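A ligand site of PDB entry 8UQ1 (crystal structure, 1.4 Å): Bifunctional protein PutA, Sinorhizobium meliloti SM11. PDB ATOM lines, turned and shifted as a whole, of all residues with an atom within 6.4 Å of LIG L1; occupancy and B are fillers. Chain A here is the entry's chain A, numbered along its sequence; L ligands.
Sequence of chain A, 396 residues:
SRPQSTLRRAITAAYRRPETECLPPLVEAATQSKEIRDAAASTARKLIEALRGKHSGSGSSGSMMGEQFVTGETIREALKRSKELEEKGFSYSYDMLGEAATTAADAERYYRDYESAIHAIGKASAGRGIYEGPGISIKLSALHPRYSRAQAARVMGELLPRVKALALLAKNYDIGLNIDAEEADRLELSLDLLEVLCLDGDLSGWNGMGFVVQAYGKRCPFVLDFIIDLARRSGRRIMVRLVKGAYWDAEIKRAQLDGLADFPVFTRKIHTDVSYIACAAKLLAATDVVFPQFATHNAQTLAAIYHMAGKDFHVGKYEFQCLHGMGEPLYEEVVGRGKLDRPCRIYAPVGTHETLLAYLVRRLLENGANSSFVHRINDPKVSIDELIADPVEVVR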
ATOM      1  N   ASP A  95      15.485  26.645   0.668  1.00  0.00           N
ATOM      2  CA  ASP A  95      16.643  27.455   1.062  1.00  0.00           C
ATOM      3  C   ASP A  95      17.273  28.028  -0.207  1.00  0.00           C
ATOM      4  O   ASP A  95      17.986  27.320  -0.923  1.00  0.00           O
ATOM      5  CB  ASP A  95      17.641  26.584   1.822  1.00  0.00           C
ATOM      6  CG  ASP A  95      18.997  27.241   1.941  1.00  0.00           C
ATOM      7  OD1 ASP A  95      19.018  28.475   2.131  1.00  0.00           O
ATOM      8  OD2 ASP A  95      20.014  26.519   1.846  1.00  0.00           O
ATOM      9  N   GLU A  99      24.973  33.187   1.418  1.00  0.00           N
ATOM     10  CA  GLU A  99      25.232  33.516   2.800  1.00  0.00           C
ATOM     11  C   GLU A  99      26.455  34.418   2.864  1.00  0.00           C
ATOM     12  O   GLU A  99      27.175  34.582   1.870  1.00  0.00           O
ATOM     13  CB  GLU A  99      25.481  32.254   3.627  1.00  0.00           C
ATOM     14  CG  GLU A  99      26.695  31.441   3.176  1.00  0.00           C
ATOM     15  CD  GLU A  99      26.756  30.087   3.857  1.00  0.00           C
ATOM     16  OE1 GLU A  99      25.816  29.284   3.697  1.00  0.00           O
ATOM     17  OE2 GLU A  99      27.743  29.838   4.569  1.00  0.00           O
ATOM     18  N   LYS A 139      18.949  32.949   5.851  1.00  0.00           N
ATOM     19  CA  LYS A 139      20.148  33.178   6.668  1.00  0.00           C
ATOM     20  C   LYS A 139      20.358  34.683   6.811  1.00  0.00           C
ATOM     21  O   LYS A 139      20.459  35.392   5.803  1.00  0.00           O
ATOM     22  CB  LYS A 139      21.374  32.536   6.017  1.00  0.00           C
ATOM     23  CG  LYS A 139      21.482  31.047   6.286  1.00  0.00           C
ATOM     24  CD  LYS A 139      22.732  30.483   5.621  1.00  0.00           C
ATOM     25  CE  LYS A 139      22.983  29.044   6.073  1.00  0.00           C
ATOM     26  NZ  LYS A 139      21.943  28.093   5.576  1.00  0.00           N
ATOM     27  N   ASP A 180      17.581  30.444   9.903  1.00  0.00           N
ATOM     28  CA  ASP A 180      18.632  29.459  10.169  1.00  0.00           C
ATOM     29  C   ASP A 180      19.602  29.972  11.240  1.00  0.00           C
ATOM     30  O   ASP A 180      19.816  31.186  11.369  1.00  0.00           O
ATOM     31  CB  ASP A 180      19.423  29.172   8.891  1.00  0.00           C
ATOM     32  CG  ASP A 180      18.698  28.278   7.886  1.00  0.00           C
ATOM     33  OD1 ASP A 180      17.616  27.747   8.177  1.00  0.00           O
ATOM     34  OD2 ASP A 180      19.224  28.099   6.776  1.00  0.00           O
ATOM     35  N   ALA A 181      20.196  29.058  12.007  1.00  0.00           N
ATOM     36  CA  ALA A 181      21.236  29.435  12.959  1.00  0.00           C
ATOM     37  C   ALA A 181      22.608  29.280  12.338  1.00  0.00           C
ATOM     38  O   ALA A 181      22.881  28.286  11.666  1.00  0.00           O
ATOM     39  CB  ALA A 181      21.161  28.542  14.204  1.00  0.00           C
ATOM     40  N   GLU A 182      23.473  30.265  12.592  1.00  0.00           N
ATOM     41  CA  GLU A 182      24.801  30.252  12.007  1.00  0.00           C
ATOM     42  C   GLU A 182      25.867  30.190  13.100  1.00  0.00           C
ATOM     43  O   GLU A 182      25.796  29.307  13.941  1.00  0.00           O
ATOM     44  CB  GLU A 182      24.937  31.413  11.019  1.00  0.00           C
ATOM     45  CG  GLU A 182      23.896  31.348   9.891  1.00  0.00           C
ATOM     46  CD  GLU A 182      24.031  32.482   8.887  1.00  0.00           C
ATOM     47  OE1 GLU A 182      24.951  32.432   8.039  1.00  0.00           O
ATOM     48  OE2 GLU A 182      23.199  33.417   8.945  1.00  0.00           O
ATOM     49  N   ARG A 241      13.133  24.816  15.291  1.00  0.00           N
ATOM     50  CA  ARG A 241      13.887  23.713  14.691  1.00  0.00           C
ATOM     51  C   ARG A 241      15.047  23.375  15.613  1.00  0.00           C
ATOM     52  O   ARG A 241      15.947  24.193  15.800  1.00  0.00           O
ATOM     53  CB  ARG A 241      14.413  24.115  13.318  1.00  0.00           C
ATOM     54  CG  ARG A 241      15.106  22.929  12.644  1.00  0.00           C
ATOM     55  CD  ARG A 241      15.941  23.315  11.446  1.00  0.00           C
ATOM     56  NE  ARG A 241      15.132  23.818  10.344  1.00  0.00           N
ATOM     57  CZ  ARG A 241      15.567  24.700   9.455  1.00  0.00           C
ATOM     58  NH1 ARG A 241      16.808  25.178   9.475  1.00  0.00           N
ATOM     59  NH2 ARG A 241      14.735  25.115   8.495  1.00  0.00           N
ATOM     60  N   ALA A 246      25.784  22.779  12.468  1.00  0.00           N
ATOM     61  CA  ALA A 246      26.516  22.556  11.226  1.00  0.00           C
ATOM     62  C   ALA A 246      27.908  23.159  11.180  1.00  0.00           C
ATOM     63  O   ALA A 246      28.624  22.917  10.206  1.00  0.00           O
ATOM     64  CB  ALA A 246      25.726  23.135  10.046  1.00  0.00           C
ATOM     65  N   TYR A 247      28.316  23.942  12.186  1.00  0.00           N
ATOM     66  CA  TYR A 247      29.558  24.703  12.134  1.00  0.00           C
ATOM     67  C   TYR A 247      30.584  24.257  13.175  1.00  0.00           C
ATOM     68  O   TYR A 247      31.451  25.048  13.557  1.00  0.00           O
ATOM     69  CB  TYR A 247      29.307  26.212  12.270  1.00  0.00           C
ATOM     70  CG  TYR A 247      28.261  26.753  11.305  1.00  0.00           C
ATOM     71  CD1 TYR A 247      26.912  26.586  11.556  1.00  0.00           C
ATOM     72  CD2 TYR A 247      28.621  27.446  10.142  1.00  0.00           C
ATOM     73  CE1 TYR A 247      25.938  27.060  10.676  1.00  0.00           C
ATOM     74  CE2 TYR A 247      27.657  27.933   9.264  1.00  0.00           C
ATOM     75  CZ  TYR A 247      26.325  27.736   9.542  1.00  0.00           C
ATOM     76  OH  TYR A 247      25.361  28.216   8.670  1.00  0.00           O
ATOM     77  N   LEU A 323      17.608  16.933   5.621  1.00  0.00           N
ATOM     78  CA  LEU A 323      18.186  17.626   4.486  1.00  0.00           C
ATOM     79  C   LEU A 323      17.945  16.835   3.199  1.00  0.00           C
ATOM     80  O   LEU A 323      18.087  15.608   3.162  1.00  0.00           O
ATOM     81  CB  LEU A 323      19.701  17.808   4.672  1.00  0.00           C
ATOM     82  CG  LEU A 323      20.170  18.629   5.869  1.00  0.00           C
ATOM     83  CD1 LEU A 323      21.692  18.772   5.905  1.00  0.00           C
ATOM     84  CD2 LEU A 323      19.516  19.991   5.891  1.00  0.00           C
ATOM     85  N   TYR A 347      14.515  20.090   4.006  1.00  0.00           N
ATOM     86  CA  TYR A 347      15.214  21.341   3.778  1.00  0.00           C
ATOM     87  C   TYR A 347      15.822  21.236   2.381  1.00  0.00           C
ATOM     88  O   TYR A 347      16.628  20.332   2.111  1.00  0.00           O
ATOM     89  CB  TYR A 347      16.274  21.514   4.866  1.00  0.00           C
ATOM     90  CG  TYR A 347      17.032  22.816   4.858  1.00  0.00           C
ATOM     91  CD1 TYR A 347      18.125  22.998   4.024  1.00  0.00           C
ATOM     92  CD2 TYR A 347      16.691  23.863   5.722  1.00  0.00           C
ATOM     93  CE1 TYR A 347      18.837  24.182   4.012  1.00  0.00           C
ATOM     94  CE2 TYR A 347      17.402  25.052   5.732  1.00  0.00           C
ATOM     95  CZ  TYR A 347      18.475  25.201   4.872  1.00  0.00           C
ATOM     96  OH  TYR A 347      19.196  26.377   4.868  1.00  0.00           O
ATOM     97  N   ALA A 358      29.664  26.774  -0.233  1.00  0.00           N
ATOM     98  CA  ALA A 358      29.824  26.855   1.218  1.00  0.00           C
ATOM     99  C   ALA A 358      28.949  25.825   1.941  1.00  0.00           C
ATOM    100  O   ALA A 358      29.367  25.216   2.932  1.00  0.00           O
ATOM    101  CB  ALA A 358      29.475  28.257   1.709  1.00  0.00           C
ATOM    102  N   TYR A 359      27.722  25.636   1.459  1.00  0.00           N
ATOM    103  CA  TYR A 359      26.847  24.619   2.012  1.00  0.00           C
ATOM    104  C   TYR A 359      27.439  23.223   1.821  1.00  0.00           C
ATOM    105  O   TYR A 359      27.418  22.402   2.741  1.00  0.00           O
ATOM    106  CB  TYR A 359      25.481  24.765   1.333  1.00  0.00           C
ATOM    107  CG  TYR A 359      24.417  23.790   1.743  1.00  0.00           C
ATOM    108  CD1 TYR A 359      24.246  22.593   1.070  1.00  0.00           C
ATOM    109  CD2 TYR A 359      23.523  24.110   2.754  1.00  0.00           C
ATOM    110  CE1 TYR A 359      23.240  21.711   1.426  1.00  0.00           C
ATOM    111  CE2 TYR A 359      22.516  23.233   3.131  1.00  0.00           C
ATOM    112  CZ  TYR A 359      22.376  22.042   2.454  1.00  0.00           C
ATOM    113  OH  TYR A 359      21.361  21.194   2.847  1.00  0.00           O
ATOM    114  N   ARG A 362      30.027  22.253   4.465  1.00  0.00           N
ATOM    115  CA  ARG A 362      29.435  21.786   5.708  1.00  0.00           C
ATOM    116  C   ARG A 362      28.870  20.372   5.549  1.00  0.00           C
ATOM    117  O   ARG A 362      28.979  19.552   6.470  1.00  0.00           O
ATOM    118  CB  ARG A 362      28.397  22.767   6.239  1.00  0.00           C
ATOM    119  CG  ARG A 362      29.020  24.086   6.678  1.00  0.00           C
ATOM    120  CD  ARG A 362      28.019  24.997   7.363  1.00  0.00           C
ATOM    121  NE  ARG A 362      26.963  25.413   6.453  1.00  0.00           N
ATOM    122  CZ  ARG A 362      27.041  26.496   5.690  1.00  0.00           C
ATOM    123  NH1 ARG A 362      28.110  27.276   5.700  1.00  0.00           N
ATOM    124  NH2 ARG A 362      26.023  26.804   4.888  1.00  0.00           N
ATOM    125  N   ARG A 363      28.298  20.058   4.389  1.00  0.00           N
ATOM    126  CA  ARG A 363      27.840  18.687   4.155  1.00  0.00           C
ATOM    127  C   ARG A 363      28.988  17.696   4.135  1.00  0.00           C
ATOM    128  O   ARG A 363      28.845  16.556   4.576  1.00  0.00           O
ATOM    129  CB  ARG A 363      27.029  18.615   2.863  1.00  0.00           C
ATOM    130  CG  ARG A 363      25.790  19.516   2.814  1.00  0.00           C
ATOM    131  CD  ARG A 363      24.665  19.105   3.793  1.00  0.00           C
ATOM    132  NE  ARG A 363      24.936  19.476   5.180  1.00  0.00           N
ATOM    133  CZ  ARG A 363      24.922  20.720   5.638  1.00  0.00           C
ATOM    134  NH1 ARG A 363      24.728  21.750   4.840  1.00  0.00           N
ATOM    135  NH2 ARG A 363      25.108  20.924   6.943  1.00  0.00           N
ATOM    136  N   GLU A 366      30.028  17.089   7.680  1.00  0.00           N
ATOM    137  CA  GLU A 366      29.000  16.272   8.323  1.00  0.00           C
ATOM    138  C   GLU A 366      29.093  14.817   7.862  1.00  0.00           C
ATOM    139  O   GLU A 366      29.121  13.894   8.685  1.00  0.00           O
ATOM    140  CB  GLU A 366      27.628  16.860   8.002  1.00  0.00           C
ATOM    141  CG  GLU A 366      26.439  16.103   8.526  1.00  0.00           C
ATOM    142  CD  GLU A 366      25.134  16.788   8.188  1.00  0.00           C
ATOM    143  OE1 GLU A 366      25.147  17.802   7.445  1.00  0.00           O
ATOM    144  OE2 GLU A 366      24.086  16.325   8.671  1.00  0.00           O
HETATM  145  C1  LIG L   1      21.867  22.351   6.635  1.00  0.00           C
HETATM  146  C2  LIG L   1      21.514  23.237   7.558  1.00  0.00           C
HETATM  147  C3  LIG L   1      20.855  24.514   7.388  1.00  0.00           C
HETATM  148  C4  LIG L   1      23.616  25.590   8.094  1.00  0.00           C
HETATM  149  C5  LIG L   1      23.959  25.021   6.647  1.00  0.00           C
HETATM  150  O1  LIG L   1      24.695  24.031   6.622  1.00  0.00           O
HETATM  151  O2  LIG L   1      23.436  25.596   5.697  1.00  0.00           O
HETATM  152  S1  LIG L   1      21.810  25.957   8.106  1.00  0.00           S
HETATM  153  P1  LG2 L   2      24.656  12.937  14.202  1.00  0.00           P
HETATM  154  O1  LG2 L   2      25.663  12.098  13.495  1.00  0.00           O
HETATM  155  O2  LG2 L   2      23.852  12.300  15.313  1.00  0.00           O
HETATM  156  O3  LG2 L   2      25.247  14.196  14.799  1.00  0.00           O
HETATM  157  C1  LG2 L   2      26.348  14.888  14.158  1.00  0.00           C
HETATM  158  C2  LG2 L   2      26.519  16.236  14.806  1.00  0.00           C
HETATM  159  O4  LG2 L   2      27.168  16.103  16.102  1.00  0.00           O
HETATM  160  C3  LG2 L   2      27.412  17.209  14.066  1.00  0.00           C
HETATM  161  O5  LG2 L   2      26.686  17.764  12.973  1.00  0.00           O
HETATM  162  C4  LG2 L   2      27.756  18.208  15.175  1.00  0.00           C
HETATM  163  O6  LG2 L   2      26.666  19.076  15.460  1.00  0.00           O
HETATM  164  C5  LG2 L   2      27.902  17.285  16.382  1.00  0.00           C
HETATM  165  N1  LG2 L   2      29.275  16.895  16.718  1.00  0.00           N
HETATM  166  C6  LG2 L   2      30.134  16.114  15.998  1.00  0.00           C
HETATM  167  N2  LG2 L   2      31.293  15.923  16.583  1.00  0.00           N
HETATM  168  C7  LG2 L   2      31.182  16.612  17.784  1.00  0.00           C
HETATM  169  C8  LG2 L   2      32.063  16.803  18.855  1.00  0.00           C
HETATM  170  N3  LG2 L   2      33.304  16.291  18.924  1.00  0.00           N
HETATM  171  N4  LG2 L   2      31.634  17.550  19.897  1.00  0.00           N
HETATM  172  C9  LG2 L   2      30.404  18.075  19.843  1.00  0.00           C
HETATM  173  N5  LG2 L   2      29.491  17.969  18.883  1.00  0.00           N
HETATM  174  C10 LG2 L   2      29.937  17.212  17.876  1.00  0.00           C
HETATM  175  N6  LG2 L   2      22.670  23.306  11.841  1.00  0.00           N
HETATM  176  C11 LG2 L   2      22.912  24.616  12.100  1.00  0.00           C
HETATM  177  O7  LG2 L   2      23.953  24.971  12.674  1.00  0.00           O
HETATM  178  N7  LG2 L   2      22.011  25.585  11.665  1.00  0.00           N
HETATM  179  C12 LG2 L   2      20.821  25.344  11.004  1.00  0.00           C
HETATM  180  O8  LG2 L   2      20.082  26.287  10.699  1.00  0.00           O
HETATM  181  C13 LG2 L   2      20.564  23.936  10.738  1.00  0.00           C
HETATM  182  N8  LG2 L   2      19.439  23.604  10.103  1.00  0.00           N
HETATM  183  C14 LG2 L   2      19.214  22.250   9.856  1.00  0.00           C
HETATM  184  C15 LG2 L   2      18.047  21.860   9.179  1.00  0.00           C
HETATM  185  C16 LG2 L   2      17.782  20.515   8.938  1.00  0.00           C
HETATM  186  C17 LG2 L   2      16.517  20.126   8.219  1.00  0.00           C
HETATM  187  C18 LG2 L   2      18.682  19.531   9.385  1.00  0.00           C
HETATM  188  C19 LG2 L   2      18.451  18.064   9.130  1.00  0.00           C
HETATM  189  C20 LG2 L   2      19.850  19.923  10.034  1.00  0.00           C
HETATM  190  C21 LG2 L   2      20.103  21.260  10.296  1.00  0.00           C
HETATM  191  N9  LG2 L   2      21.294  21.667  10.933  1.00  0.00           N
HETATM  192  C22 LG2 L   2      21.535  22.989  11.207  1.00  0.00           C
HETATM  193  C23 LG2 L   2      22.194  20.658  11.520  1.00  0.00           C
HETATM  194  C24 LG2 L   2      23.374  20.240  10.663  1.00  0.00           C
HETATM  195  O9  LG2 L   2      23.237  20.662   9.306  1.00  0.00           O
HETATM  196  C25 LG2 L   2      23.504  18.711  10.688  1.00  0.00           C
HETATM  197  O10 LG2 L   2      22.599  18.104   9.778  1.00  0.00           O
HETATM  198  C26 LG2 L   2      23.304  18.037  12.048  1.00  0.00           C
HETATM  199  O11 LG2 L   2      24.055  18.693  13.073  1.00  0.00           O
HETATM  200  C27 LG2 L   2      23.592  16.548  12.001  1.00  0.00           C
HETATM  201  O12 LG2 L   2      22.976  15.920  13.146  1.00  0.00           O
HETATM  202  P2  LG2 L   2      22.366  14.483  13.047  1.00  0.00           P
HETATM  203  O13 LG2 L   2      21.529  14.331  14.333  1.00  0.00           O
HETATM  204  O14 LG2 L   2      21.725  14.264  11.790  1.00  0.00           O
HETATM  205  O15 LG2 L   2      23.650  13.527  13.130  1.00  0.00           O
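The guanidinium group (NH1) of Arg 241 lies within hydrogen-bond range of a nitrogen (N8) of LG2 L2 (3.1 Å). NE of Arg 362 lies within salt-bridge range of O1 of LIG L1 (2.7 Å). An oxygen (O9) of LG2 L2 sits at hydrogen-bond distance from the guanidinium group of Arg 363 (3.0 Å). The side-chain amino group of Lys 139 lies within salt-bridge range of an oxygen (O2) of LIG L1 (2.9 Å). N of Ala 246 lies within hydrogen-bond range of O7 of LG2 L2 (2.9 Å). OE2 of Glu 366 sits at hydrogen-bond distance from O10 of LG2 L2. NH1 of Arg 363 is in salt-bridge range of O1 of LIG L1, 2.9 Å away. The backbone NH (N) of Ala 181 lies within hydrogen-bond range of an oxygen (O8) of LG2 L2 (3.1 Å). The backbone carbonyl oxygen (O) of Ala 181 lies within hydrogen-bond range of a nitrogen (N7) of LG2 L2 (2.8 Å).
A nitrogen (N7) of LG2 L2 lies close to a sulfur (S1) of LIG L1 (3.6 Å).
The side-chain hydroxyl (OH) of Tyr 347 lies close to the side-chain carboxylate (OD2) of Asp 95. OD1 of Asp 180 lies within salt-bridge range of NH1 of Arg 241 (3.0 Å). The backbone carbonyl oxygen of Tyr 359 sits close to the guanidinium group of Arg 363. The guanidinium group (NE) of Arg 363 is in salt-bridge range of the side-chain carboxylate (OE1) of Glu 366, 2.8 Å away. The side-chain hydroxyl (OH) of Tyr 347 is in hydrogen-bond range of the side-chain amino group (NZ) of Lys 139 (3.3 Å). The side-chain amino group of Lys 139 lies within salt-bridge range of the side-chain carboxylate of Asp 180. NH2 of Arg 362 lies within salt-bridge range of OE1 of Glu 99. The side-chain carboxylate (OD2) of Asp 180 sits at hydrogen-bond distance from the side-chain hydroxyl (OH) of Tyr 347, 2.6 Å away.
The side-chain carboxylate (OD2) of Asp 180 lies close to a sulfur (S1) of LIG L1 (3.6 Å). Merely in contact with LIG L1: Tyr 247, Tyr 359, Leu 323, Tyr 347 and Ala 246. Nine residues have an atom within 4 Å of LIG L1: Lys 139, Asp 180, Ala 246, Tyr 247, Leu 323, Tyr 347, Tyr 359, Arg 362 and Arg 363.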
